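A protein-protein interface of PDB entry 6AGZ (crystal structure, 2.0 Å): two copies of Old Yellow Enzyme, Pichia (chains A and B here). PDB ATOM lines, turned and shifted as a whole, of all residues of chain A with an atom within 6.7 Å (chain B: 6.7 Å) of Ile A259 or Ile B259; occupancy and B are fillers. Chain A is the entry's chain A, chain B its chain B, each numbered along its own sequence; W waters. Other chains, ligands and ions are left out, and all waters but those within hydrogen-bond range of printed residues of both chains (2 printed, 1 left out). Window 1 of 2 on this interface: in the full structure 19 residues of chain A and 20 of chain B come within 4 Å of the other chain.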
ATOM      1  N   PRO A 242       6.200  21.246 -16.785  1.00  0.00           N
ATOM      2  CA  PRO A 242       4.919  21.118 -16.067  1.00  0.00           C
ATOM      3  C   PRO A 242       4.455  22.396 -15.388  1.00  0.00           C
ATOM      4  O   PRO A 242       3.243  22.638 -15.316  1.00  0.00           O
ATOM      5  CB  PRO A 242       5.205  20.012 -15.040  1.00  0.00           C
ATOM      6  CG  PRO A 242       6.378  19.265 -15.593  1.00  0.00           C
ATOM      7  CD  PRO A 242       7.208  20.294 -16.291  1.00  0.00           C
ATOM      8  N   TYR A 243       5.372  23.224 -14.887  1.00  0.00           N
ATOM      9  CA  TYR A 243       4.999  24.417 -14.140  1.00  0.00           C
ATOM     10  C   TYR A 243       4.839  25.658 -15.007  1.00  0.00           C
ATOM     11  O   TYR A 243       4.321  26.669 -14.520  1.00  0.00           O
ATOM     12  CB  TYR A 243       6.037  24.708 -13.050  1.00  0.00           C
ATOM     13  CG  TYR A 243       6.088  23.677 -11.948  1.00  0.00           C
ATOM     14  CD1 TYR A 243       5.034  23.533 -11.056  1.00  0.00           C
ATOM     15  CD2 TYR A 243       7.196  22.855 -11.790  1.00  0.00           C
ATOM     16  CE1 TYR A 243       5.078  22.595 -10.044  1.00  0.00           C
ATOM     17  CE2 TYR A 243       7.249  21.914 -10.781  1.00  0.00           C
ATOM     18  CZ  TYR A 243       6.187  21.787  -9.911  1.00  0.00           C
ATOM     19  OH  TYR A 243       6.234  20.853  -8.903  1.00  0.00           O
ATOM     20  N   VAL A 256      -6.615  20.108 -13.663  1.00  0.00           N
ATOM     21  CA  VAL A 256      -5.958  18.915 -13.148  1.00  0.00           C
ATOM     22  C   VAL A 256      -4.492  19.259 -12.927  1.00  0.00           C
ATOM     23  O   VAL A 256      -3.831  19.778 -13.834  1.00  0.00           O
ATOM     24  CB  VAL A 256      -6.114  17.721 -14.106  1.00  0.00           C
ATOM     25  CG1 VAL A 256      -5.364  16.508 -13.571  1.00  0.00           C
ATOM     26  CG2 VAL A 256      -7.583  17.389 -14.307  1.00  0.00           C
ATOM     27  N   HIS A 257      -3.992  18.971 -11.729  1.00  0.00           N
ATOM     28  CA  HIS A 257      -2.665  19.429 -11.338  1.00  0.00           C
ATOM     29  C   HIS A 257      -1.598  18.822 -12.249  1.00  0.00           C
ATOM     30  O   HIS A 257      -1.705  17.653 -12.639  1.00  0.00           O
ATOM     31  CB  HIS A 257      -2.387  19.057  -9.879  1.00  0.00           C
ATOM     32  CG  HIS A 257      -1.306  19.869  -9.237  1.00  0.00           C
ATOM     33  ND1 HIS A 257       0.032  19.571  -9.376  1.00  0.00           N
ATOM     34  CD2 HIS A 257      -1.365  20.970  -8.451  1.00  0.00           C
ATOM     35  CE1 HIS A 257       0.750  20.453  -8.705  1.00  0.00           C
ATOM     36  NE2 HIS A 257      -0.074  21.312  -8.133  1.00  0.00           N
ATOM     37  N   PRO A 258      -0.565  19.588 -12.614  1.00  0.00           N
ATOM     38  CA  PRO A 258       0.464  19.051 -13.523  1.00  0.00           C
ATOM     39  C   PRO A 258       1.261  17.899 -12.940  1.00  0.00           C
ATOM     40  O   PRO A 258       1.881  17.151 -13.705  1.00  0.00           O
ATOM     41  CB  PRO A 258       1.359  20.269 -13.794  1.00  0.00           C
ATOM     42  CG  PRO A 258       1.123  21.182 -12.630  1.00  0.00           C
ATOM     43  CD  PRO A 258      -0.321  20.999 -12.273  1.00  0.00           C
ATOM     44  N   ILE A 259       1.282  17.737 -11.615  1.00  0.00           N
ATOM     45  CA  ILE A 259       1.963  16.586 -11.029  1.00  0.00           C
ATOM     46  C   ILE A 259       1.266  15.294 -11.435  1.00  0.00           C
ATOM     47  O   ILE A 259       1.918  14.262 -11.639  1.00  0.00           O
ATOM     48  CB  ILE A 259       2.054  16.747  -9.497  1.00  0.00           C
ATOM     49  CG1 ILE A 259       3.048  17.858  -9.144  1.00  0.00           C
ATOM     50  CG2 ILE A 259       2.462  15.444  -8.828  1.00  0.00           C
ATOM     51  CD1 ILE A 259       3.176  18.123  -7.658  1.00  0.00           C
ATOM     52  N   ALA A 260      -0.059  15.330 -11.585  1.00  0.00           N
ATOM     53  CA  ALA A 260      -0.803  14.150 -12.018  1.00  0.00           C
ATOM     54  C   ALA A 260      -0.648  13.905 -13.514  1.00  0.00           C
ATOM     55  O   ALA A 260      -0.345  12.787 -13.941  1.00  0.00           O
ATOM     56  CB  ALA A 260      -2.281  14.302 -11.656  1.00  0.00           C
ATOM     57  N   GLN A 261      -0.874  14.941 -14.322  1.00  0.00           N
ATOM     58  CA  GLN A 261      -0.787  14.810 -15.775  1.00  0.00           C
ATOM     59  C   GLN A 261       0.626  14.430 -16.210  1.00  0.00           C
ATOM     60  O   GLN A 261       0.857  13.361 -16.795  1.00  0.00           O
ATOM     61  CB  GLN A 261      -1.223  16.131 -16.414  1.00  0.00           C
ATOM     62  CG  GLN A 261      -1.216  16.162 -17.926  1.00  0.00           C
ATOM     63  CD  GLN A 261      -2.322  15.332 -18.541  1.00  0.00           C
ATOM     64  OE1 GLN A 261      -3.503  15.656 -18.414  1.00  0.00           O
ATOM     65  NE2 GLN A 261      -1.942  14.264 -19.228  1.00  0.00           N
ATOM     66  N   PHE A 262       1.592  15.299 -15.909  1.00  0.00           N
ATOM     67  CA  PHE A 262       2.976  15.027 -16.275  1.00  0.00           C
ATOM     68  C   PHE A 262       3.562  13.890 -15.450  1.00  0.00           C
ATOM     69  O   PHE A 262       4.497  13.221 -15.901  1.00  0.00           O
ATOM     70  CB  PHE A 262       3.811  16.295 -16.122  1.00  0.00           C
ATOM     71  CG  PHE A 262       3.383  17.407 -17.036  1.00  0.00           C
ATOM     72  CD1 PHE A 262       3.997  17.584 -18.263  1.00  0.00           C
ATOM     73  CD2 PHE A 262       2.356  18.264 -16.674  1.00  0.00           C
ATOM     74  CE1 PHE A 262       3.602  18.602 -19.110  1.00  0.00           C
ATOM     75  CE2 PHE A 262       1.956  19.284 -17.518  1.00  0.00           C
ATOM     76  CZ  PHE A 262       2.580  19.453 -18.737  1.00  0.00           C
ATOM     77  N   GLY A 263       3.038  13.661 -14.245  1.00  0.00           N
ATOM     78  CA  GLY A 263       3.403  12.458 -13.515  1.00  0.00           C
ATOM     79  C   GLY A 263       3.040  11.200 -14.281  1.00  0.00           C
ATOM     80  O   GLY A 263       3.814  10.239 -14.326  1.00  0.00           O
ATOM     81  N   TYR A 264       1.859  11.196 -14.907  1.00  0.00           N
ATOM     82  CA  TYR A 264       1.473  10.070 -15.750  1.00  0.00           C
ATOM     83  C   TYR A 264       2.361   9.974 -16.982  1.00  0.00           C
ATOM     84  O   TYR A 264       2.747   8.870 -17.386  1.00  0.00           O
ATOM     85  CB  TYR A 264       0.005  10.189 -16.156  1.00  0.00           C
ATOM     86  CG  TYR A 264      -0.387   9.275 -17.300  1.00  0.00           C
ATOM     87  CD1 TYR A 264      -0.710   7.943 -17.074  1.00  0.00           C
ATOM     88  CD2 TYR A 264      -0.435   9.746 -18.607  1.00  0.00           C
ATOM     89  CE1 TYR A 264      -1.066   7.106 -18.117  1.00  0.00           C
ATOM     90  CE2 TYR A 264      -0.787   8.918 -19.655  1.00  0.00           C
ATOM     91  CZ  TYR A 264      -1.103   7.600 -19.406  1.00  0.00           C
ATOM     92  OH  TYR A 264      -1.455   6.776 -20.449  1.00  0.00           O
ATOM     93  N   ASP A 301       8.778  22.345  -7.276  1.00  0.00           N
ATOM     94  CA  ASP A 301      10.047  21.636  -7.191  1.00  0.00           C
ATOM     95  C   ASP A 301       9.957  20.382  -8.049  1.00  0.00           C
ATOM     96  O   ASP A 301       8.946  19.677  -8.013  1.00  0.00           O
ATOM     97  CB  ASP A 301      10.387  21.274  -5.742  1.00  0.00           C
ATOM     98  CG  ASP A 301      11.817  20.800  -5.580  1.00  0.00           C
ATOM     99  OD1 ASP A 301      12.111  19.649  -5.963  1.00  0.00           O
ATOM    100  OD2 ASP A 301      12.648  21.577  -5.066  1.00  0.00           O
ATOM    101  N   SER A 303      11.595  17.593  -7.848  1.00  0.00           N
ATOM    102  CA  SER A 303      12.059  16.356  -7.225  1.00  0.00           C
ATOM    103  C   SER A 303      11.177  15.172  -7.596  1.00  0.00           C
ATOM    104  O   SER A 303      11.681  14.094  -7.937  1.00  0.00           O
ATOM    105  CB  SER A 303      12.112  16.521  -5.705  1.00  0.00           C
ATOM    106  OG  SER A 303      10.841  16.875  -5.189  1.00  0.00           O
ATOM    107  N   TRP A 304       9.853  15.362  -7.562  1.00  0.00           N
ATOM    108  CA  TRP A 304       8.937  14.272  -7.878  1.00  0.00           C
ATOM    109  C   TRP A 304       9.203  13.710  -9.268  1.00  0.00           C
ATOM    110  O   TRP A 304       9.125  12.494  -9.477  1.00  0.00           O
ATOM    111  CB  TRP A 304       7.489  14.748  -7.761  1.00  0.00           C
ATOM    112  CG  TRP A 304       7.160  15.912  -8.646  1.00  0.00           C
ATOM    113  CD1 TRP A 304       7.295  17.234  -8.341  1.00  0.00           C
ATOM    114  CD2 TRP A 304       6.634  15.859  -9.979  1.00  0.00           C
ATOM    115  NE1 TRP A 304       6.891  18.009  -9.401  1.00  0.00           N
ATOM    116  CE2 TRP A 304       6.480  17.189 -10.419  1.00  0.00           C
ATOM    117  CE3 TRP A 304       6.281  14.818 -10.842  1.00  0.00           C
ATOM    118  CZ2 TRP A 304       5.986  17.506 -11.683  1.00  0.00           C
ATOM    119  CZ3 TRP A 304       5.792  15.134 -12.099  1.00  0.00           C
ATOM    120  CH2 TRP A 304       5.649  16.466 -12.507  1.00  0.00           C
ATOM    121  N   MET A 305       9.532  14.580 -10.227  1.00  0.00           N
ATOM    122  CA  MET A 305       9.876  14.104 -11.562  1.00  0.00           C
ATOM    123  C   MET A 305      11.011  13.092 -11.493  1.00  0.00           C
ATOM    124  O   MET A 305      10.914  11.988 -12.047  1.00  0.00           O
ATOM    125  CB  MET A 305      10.252  15.282 -12.463  1.00  0.00           C
ATOM    126  CG  MET A 305       9.192  16.370 -12.524  1.00  0.00           C
ATOM    127  SD  MET A 305       9.536  17.664 -13.736  1.00  0.00           S
ATOM    128  CE  MET A 305       9.116  16.818 -15.257  1.00  0.00           C
ATOM    129  N   GLN A 307      11.761  11.275  -9.116  1.00  0.00           N
ATOM    130  CA  GLN A 307      11.291  10.047  -8.484  1.00  0.00           C
ATOM    131  C   GLN A 307      10.781   9.050  -9.514  1.00  0.00           C
ATOM    132  O   GLN A 307      10.935   7.838  -9.331  1.00  0.00           O
ATOM    133  CB  GLN A 307      10.184  10.350  -7.473  1.00  0.00           C
ATOM    134  CG  GLN A 307      10.665  10.872  -6.133  1.00  0.00           C
ATOM    135  CD  GLN A 307       9.582  10.801  -5.071  1.00  0.00           C
ATOM    136  OE1 GLN A 307       9.296  11.786  -4.390  1.00  0.00           O
ATOM    137  NE2 GLN A 307       8.975   9.629  -4.925  1.00  0.00           N
ATOM    138  N   ILE A 308      10.178   9.537 -10.599  1.00  0.00           N
ATOM    139  CA  ILE A 308       9.497   8.663 -11.546  1.00  0.00           C
ATOM    140  C   ILE A 308      10.465   8.226 -12.636  1.00  0.00           C
ATOM    141  O   ILE A 308      10.666   7.027 -12.860  1.00  0.00           O
ATOM    142  CB  ILE A 308       8.264   9.359 -12.149  1.00  0.00           C
ATOM    143  CG1 ILE A 308       7.348   9.868 -11.035  1.00  0.00           C
ATOM    144  CG2 ILE A 308       7.514   8.402 -13.055  1.00  0.00           C
ATOM    145  CD1 ILE A 308       6.211  10.735 -11.524  1.00  0.00           C
ATOM    146  N   PRO B 242       0.200   6.235  -0.654  1.00  0.00           N
ATOM    147  CA  PRO B 242       0.687   6.009  -2.026  1.00  0.00           C
ATOM    148  C   PRO B 242       1.897   5.092  -2.111  1.00  0.00           C
ATOM    149  O   PRO B 242       2.058   4.393  -3.118  1.00  0.00           O
ATOM    150  CB  PRO B 242       1.022   7.426  -2.514  1.00  0.00           C
ATOM    151  CG  PRO B 242       0.206   8.332  -1.649  1.00  0.00           C
ATOM    152  CD  PRO B 242       0.165   7.666  -0.308  1.00  0.00           C
ATOM    153  N   TYR B 243       2.754   5.073  -1.091  1.00  0.00           N
ATOM    154  CA  TYR B 243       3.971   4.273  -1.135  1.00  0.00           C
ATOM    155  C   TYR B 243       3.825   2.904  -0.482  1.00  0.00           C
ATOM    156  O   TYR B 243       4.715   2.062  -0.650  1.00  0.00           O
ATOM    157  CB  TYR B 243       5.125   5.024  -0.460  1.00  0.00           C
ATOM    158  CG  TYR B 243       5.590   6.251  -1.210  1.00  0.00           C
ATOM    159  CD1 TYR B 243       6.288   6.134  -2.403  1.00  0.00           C
ATOM    160  CD2 TYR B 243       5.342   7.525  -0.718  1.00  0.00           C
ATOM    161  CE1 TYR B 243       6.720   7.252  -3.091  1.00  0.00           C
ATOM    162  CE2 TYR B 243       5.770   8.648  -1.399  1.00  0.00           C
ATOM    163  CZ  TYR B 243       6.459   8.505  -2.584  1.00  0.00           C
ATOM    164  OH  TYR B 243       6.887   9.622  -3.265  1.00  0.00           O
ATOM    165  N   VAL B 256       1.134   2.103 -13.178  1.00  0.00           N
ATOM    166  CA  VAL B 256       1.068   3.558 -13.221  1.00  0.00           C
ATOM    167  C   VAL B 256       1.603   4.081 -11.896  1.00  0.00           C
ATOM    168  O   VAL B 256       1.152   3.651 -10.827  1.00  0.00           O
ATOM    169  CB  VAL B 256      -0.365   4.052 -13.483  1.00  0.00           C
ATOM    170  CG1 VAL B 256      -0.428   5.568 -13.412  1.00  0.00           C
ATOM    171  CG2 VAL B 256      -0.855   3.556 -14.838  1.00  0.00           C
ATOM    172  N   HIS B 257       2.563   4.998 -11.967  1.00  0.00           N
ATOM    173  CA  HIS B 257       3.270   5.423 -10.767  1.00  0.00           C
ATOM    174  C   HIS B 257       2.305   6.093  -9.790  1.00  0.00           C
ATOM    175  O   HIS B 257       1.424   6.855 -10.209  1.00  0.00           O
ATOM    176  CB  HIS B 257       4.409   6.379 -11.128  1.00  0.00           C
ATOM    177  CG  HIS B 257       5.425   6.544 -10.041  1.00  0.00           C
ATOM    178  ND1 HIS B 257       5.231   7.373  -8.958  1.00  0.00           N
ATOM    179  CD2 HIS B 257       6.642   5.976  -9.867  1.00  0.00           C
ATOM    180  CE1 HIS B 257       6.285   7.312  -8.165  1.00  0.00           C
ATOM    181  NE2 HIS B 257       7.157   6.473  -8.695  1.00  0.00           N
ATOM    182  N   PRO B 258       2.437   5.828  -8.487  1.00  0.00           N
ATOM    183  CA  PRO B 258       1.493   6.406  -7.515  1.00  0.00           C
ATOM    184  C   PRO B 258       1.482   7.925  -7.483  1.00  0.00           C
ATOM    185  O   PRO B 258       0.492   8.509  -7.027  1.00  0.00           O
ATOM    186  CB  PRO B 258       1.964   5.821  -6.175  1.00  0.00           C
ATOM    187  CG  PRO B 258       3.377   5.364  -6.422  1.00  0.00           C
ATOM    188  CD  PRO B 258       3.402   4.919  -7.849  1.00  0.00           C
ATOM    189  N   ILE B 259       2.548   8.587  -7.941  1.00  0.00           N
ATOM    190  CA  ILE B 259       2.533  10.046  -8.005  1.00  0.00           C
ATOM    191  C   ILE B 259       1.472  10.522  -8.990  1.00  0.00           C
ATOM    192  O   ILE B 259       0.803  11.539  -8.766  1.00  0.00           O
ATOM    193  CB  ILE B 259       3.934  10.579  -8.365  1.00  0.00           C
ATOM    194  CG1 ILE B 259       4.919  10.283  -7.232  1.00  0.00           C
ATOM    195  CG2 ILE B 259       3.894  12.071  -8.646  1.00  0.00           C
ATOM    196  CD1 ILE B 259       6.332  10.747  -7.513  1.00  0.00           C
ATOM    197  N   ALA B 260       1.280   9.780 -10.083  1.00  0.00           N
ATOM    198  CA  ALA B 260       0.253  10.141 -11.055  1.00  0.00           C
ATOM    199  C   ALA B 260      -1.143   9.847 -10.517  1.00  0.00           C
ATOM    200  O   ALA B 260      -2.044  10.690 -10.600  1.00  0.00           O
ATOM    201  CB  ALA B 260       0.492   9.395 -12.366  1.00  0.00           C
ATOM    202  N   GLN B 261      -1.336   8.653  -9.955  1.00  0.00           N
ATOM    203  CA  GLN B 261      -2.659   8.230  -9.507  1.00  0.00           C
ATOM    204  C   GLN B 261      -3.109   9.028  -8.288  1.00  0.00           C
ATOM    205  O   GLN B 261      -4.112   9.758  -8.333  1.00  0.00           O
ATOM    206  CB  GLN B 261      -2.629   6.731  -9.198  1.00  0.00           C
ATOM    207  CG  GLN B 261      -3.925   6.165  -8.659  1.00  0.00           C
ATOM    208  CD  GLN B 261      -5.007   6.099  -9.712  1.00  0.00           C
ATOM    209  OE1 GLN B 261      -4.860   5.418 -10.726  1.00  0.00           O
ATOM    210  NE2 GLN B 261      -6.101   6.813  -9.480  1.00  0.00           N
ATOM    211  N   PHE B 262      -2.369   8.908  -7.185  1.00  0.00           N
ATOM    212  CA  PHE B 262      -2.683   9.679  -5.991  1.00  0.00           C
ATOM    213  C   PHE B 262      -2.477  11.170  -6.210  1.00  0.00           C
ATOM    214  O   PHE B 262      -3.098  11.977  -5.510  1.00  0.00           O
ATOM    215  CB  PHE B 262      -1.841   9.190  -4.814  1.00  0.00           C
ATOM    216  CG  PHE B 262      -2.145   7.778  -4.403  1.00  0.00           C
ATOM    217  CD1 PHE B 262      -3.036   7.521  -3.374  1.00  0.00           C
ATOM    218  CD2 PHE B 262      -1.548   6.708  -5.050  1.00  0.00           C
ATOM    219  CE1 PHE B 262      -3.323   6.226  -2.996  1.00  0.00           C
ATOM    220  CE2 PHE B 262      -1.831   5.408  -4.676  1.00  0.00           C
ATOM    221  CZ  PHE B 262      -2.719   5.166  -3.647  1.00  0.00           C
ATOM    222  N   GLY B 263      -1.622  11.552  -7.161  1.00  0.00           N
ATOM    223  CA  GLY B 263      -1.572  12.944  -7.569  1.00  0.00           C
ATOM    224  C   GLY B 263      -2.896  13.420  -8.134  1.00  0.00           C
ATOM    225  O   GLY B 263      -3.358  14.522  -7.824  1.00  0.00           O
ATOM    226  N   TYR B 264      -3.531  12.590  -8.967  1.00  0.00           N
ATOM    227  CA  TYR B 264      -4.862  12.921  -9.465  1.00  0.00           C
ATOM    228  C   TYR B 264      -5.874  12.984  -8.330  1.00  0.00           C
ATOM    229  O   TYR B 264      -6.725  13.880  -8.301  1.00  0.00           O
ATOM    230  CB  TYR B 264      -5.309  11.903 -10.512  1.00  0.00           C
ATOM    231  CG  TYR B 264      -6.775  12.019 -10.884  1.00  0.00           C
ATOM    232  CD1 TYR B 264      -7.209  12.984 -11.783  1.00  0.00           C
ATOM    233  CD2 TYR B 264      -7.723  11.164 -10.333  1.00  0.00           C
ATOM    234  CE1 TYR B 264      -8.544  13.095 -12.124  1.00  0.00           C
ATOM    235  CE2 TYR B 264      -9.061  11.269 -10.668  1.00  0.00           C
ATOM    236  CZ  TYR B 264      -9.464  12.235 -11.565  1.00  0.00           C
ATOM    237  OH  TYR B 264     -10.794  12.343 -11.902  1.00  0.00           O
ATOM    238  N   ASP B 301       9.204  10.324  -1.001  1.00  0.00           N
ATOM    239  CA  ASP B 301       9.038  11.603  -0.321  1.00  0.00           C
ATOM    240  C   ASP B 301       7.644  12.134  -0.621  1.00  0.00           C
ATOM    241  O   ASP B 301       7.208  12.106  -1.775  1.00  0.00           O
ATOM    242  CB  ASP B 301      10.114  12.603  -0.770  1.00  0.00           C
ATOM    243  CG  ASP B 301      10.166  13.849   0.099  1.00  0.00           C
ATOM    244  OD1 ASP B 301       9.103  14.445   0.371  1.00  0.00           O
ATOM    245  OD2 ASP B 301      11.279  14.234   0.513  1.00  0.00           O
ATOM    246  N   SER B 303       6.564  15.226  -0.447  1.00  0.00           N
ATOM    247  CA  SER B 303       6.536  16.672  -0.651  1.00  0.00           C
ATOM    248  C   SER B 303       5.569  17.065  -1.763  1.00  0.00           C
ATOM    249  O   SER B 303       4.892  18.098  -1.669  1.00  0.00           O
ATOM    250  CB  SER B 303       7.945  17.188  -0.950  1.00  0.00           C
ATOM    251  OG  SER B 303       8.570  16.421  -1.963  1.00  0.00           O
ATOM    252  N   TRP B 304       5.490  16.257  -2.824  1.00  0.00           N
ATOM    253  CA  TRP B 304       4.550  16.543  -3.905  1.00  0.00           C
ATOM    254  C   TRP B 304       3.112  16.559  -3.398  1.00  0.00           C
ATOM    255  O   TRP B 304       2.297  17.385  -3.835  1.00  0.00           O
ATOM    256  CB  TRP B 304       4.721  15.518  -5.028  1.00  0.00           C
ATOM    257  CG  TRP B 304       4.584  14.090  -4.580  1.00  0.00           C
ATOM    258  CD1 TRP B 304       5.575  13.280  -4.107  1.00  0.00           C
ATOM    259  CD2 TRP B 304       3.385  13.303  -4.573  1.00  0.00           C
ATOM    260  NE1 TRP B 304       5.068  12.039  -3.800  1.00  0.00           N
ATOM    261  CE2 TRP B 304       3.726  12.027  -4.078  1.00  0.00           C
ATOM    262  CE3 TRP B 304       2.058  13.554  -4.935  1.00  0.00           C
ATOM    263  CZ2 TRP B 304       2.787  11.007  -3.937  1.00  0.00           C
ATOM    264  CZ3 TRP B 304       1.128  12.539  -4.794  1.00  0.00           C
ATOM    265  CH2 TRP B 304       1.497  11.281  -4.300  1.00  0.00           C
ATOM    266  N   MET B 305       2.785  15.654  -2.469  1.00  0.00           N
ATOM    267  CA  MET B 305       1.456  15.649  -1.870  1.00  0.00           C
ATOM    268  C   MET B 305       1.123  17.004  -1.262  1.00  0.00           C
ATOM    269  O   MET B 305       0.005  17.508  -1.421  1.00  0.00           O
ATOM    270  CB  MET B 305       1.358  14.551  -0.810  1.00  0.00           C
ATOM    271  CG  MET B 305       1.787  13.173  -1.288  1.00  0.00           C
ATOM    272  SD  MET B 305       1.350  11.862  -0.126  1.00  0.00           S
ATOM    273  CE  MET B 305      -0.414  11.739  -0.411  1.00  0.00           C
ATOM    274  N   GLN B 307       2.554  19.768  -2.228  1.00  0.00           N
ATOM    275  CA  GLN B 307       2.439  20.692  -3.350  1.00  0.00           C
ATOM    276  C   GLN B 307       1.011  20.739  -3.873  1.00  0.00           C
ATOM    277  O   GLN B 307       0.527  21.799  -4.287  1.00  0.00           O
ATOM    278  CB  GLN B 307       3.393  20.300  -4.477  1.00  0.00           C
ATOM    279  CG  GLN B 307       4.861  20.544  -4.192  1.00  0.00           C
ATOM    280  CD  GLN B 307       5.695  20.547  -5.459  1.00  0.00           C
ATOM    281  OE1 GLN B 307       6.681  19.821  -5.570  1.00  0.00           O
ATOM    282  NE2 GLN B 307       5.298  21.368  -6.424  1.00  0.00           N
ATOM    283  N   ILE B 308       0.317  19.602  -3.857  1.00  0.00           N
ATOM    284  CA  ILE B 308      -1.020  19.534  -4.439  1.00  0.00           C
ATOM    285  C   ILE B 308      -2.077  19.959  -3.424  1.00  0.00           C
ATOM    286  O   ILE B 308      -2.844  20.896  -3.671  1.00  0.00           O
ATOM    287  CB  ILE B 308      -1.312  18.127  -4.983  1.00  0.00           C
ATOM    288  CG1 ILE B 308      -0.259  17.740  -6.024  1.00  0.00           C
ATOM    289  CG2 ILE B 308      -2.694  18.085  -5.600  1.00  0.00           C
ATOM    290  CD1 ILE B 308      -0.406  16.333  -6.549  1.00  0.00           C
HETATM  291  O   HOH W   1       0.894  23.163  -6.424  1.00  0.00           O
HETATM  292  O   HOH W   2       9.598   6.040  -7.504  1.00  0.00           O
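His A257 touches Ile B308, and with the chains exchanged Ile A308 touches His B257.
Ile A259 touches Trp B304, and with the chains exchanged Trp A304 touches Ile B259.
Ile A259 touches Ile B308, and with the chains exchanged Ile A308 touches Ile B259.
Ser B303 touches its own counterpart, Ser A303.
Positions printed for both chains: 242, 243, 256, 257, 258, 259, 260, 261, 262, 263, 264, 301, 303, 304, 305, 307 and 308.
Of the 17 printed residues of chain B, 11 touch a printed residue of chain A.
Among the printed residues, 22 pairs touch across the chains.
The backbone carbonyl oxygen of Asp A301 sits close to the side-chain amide oxygen of Gln B307.
The side-chain amide oxygen of Gln A307 sits close to the backbone carbonyl oxygen of Asp B301 (3.4 Å).
The side-chain amide nitrogen (NE2) of Gln A307 lies within hydrogen-bond range of the side-chain hydroxyl (OH) of Tyr B243, 2.7 Å away.
The side-chain hydroxyl of Tyr A243 is in hydrogen-bond range of the side-chain amide nitrogen of Gln B307, at 2.7 Å.
Water W1 bridges the backbone carbonyl oxygen (O) of Gln B307 (2.6 Å) and a ring nitrogen (NE2) of His A257 (2.7 Å).
Water W2 bridges a ring nitrogen (NE2) of His B257 and the backbone carbonyl oxygen (O) of Gln A307.
Of the printed residues of chain B, Ile A259 touches Ile B259 (3.7 Å), Trp B304 (3.99 Å), Gln B307 (3.9 Å) and Ile B308 (3.8 Å).
Printed residues of chain A within 4 Å of Ile B259: Ile A259, Trp A304, Gln A307 and Ile A308.
Printed residues of chain A within 4 Å of Ala B260: Ala A260, Gly A263 and Tyr A264.
Of the printed residues of chain A, Trp B304 touches Ile A259 and Trp A304.
Printed residues of chain A within 4 Å of Ile B308: His A257 and Ile A259.
Of the printed residues of chain A, Tyr B243 touches Gln A307.
Printed residues of chain A within 4 Å of Gly B263: Ala A260 (3.7 Å).
The nearest printed residue of chain A that does not touch His B257 is Gln A307 (4.1 Å).
Among the printed residues, pairs that only touch across the chains: His A257 with Gln B307 (3.9 Å), His A257 with Ile B308 (3.8 Å), Ile A259 with Ile B259 (3.7 Å), Ile A259 with Trp B304 (3.99 Å), Ile A259 with Gln B307 (3.9 Å), Ile A259 with Ile B308 (3.8 Å), Ala A260 with Ala B260 (3.8 Å), Ala A260 with Gly B263 (3.7 Å), Ala A260 with Tyr B264 (3.4 Å), Gly A263 with Ala B260 (3.7 Å), Tyr A264 with Ala B260 (3.4 Å), Ser A303 with Ser B303 (3.97 Å), Trp A304 with Ile B259 (3.8 Å), Trp A304 with Trp B304 (3.97 Å), Trp A304 with Gln B307 (3.8 Å), Gln A307 with Ile B259 (3.9 Å), Ile A308 with His B257 (3.9 Å) and Ile A308 with Ile B259 (3.8 Å).
OH of Tyr B243 sits at hydrogen-bond distance from NE1 of Trp B304, 3.1 Å away.
O of Asp B301 is in hydrogen-bond range of NE1 of Trp B304.
A ring nitrogen (ND1) of His A257 sits close to the backbone NH (N) of Ile A259 (3.2 Å).
The side-chain hydroxyl (OH) of Tyr A243 sits at hydrogen-bond distance from the indole nitrogen (NE1) of Trp A304 (3.0 Å).
O of Asp B301 sits at hydrogen-bond distance from OH of Tyr B243 (2.9 Å).
The backbone NH of Ile B259 sits close to a ring nitrogen (ND1) of His B257 (3.1 Å).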
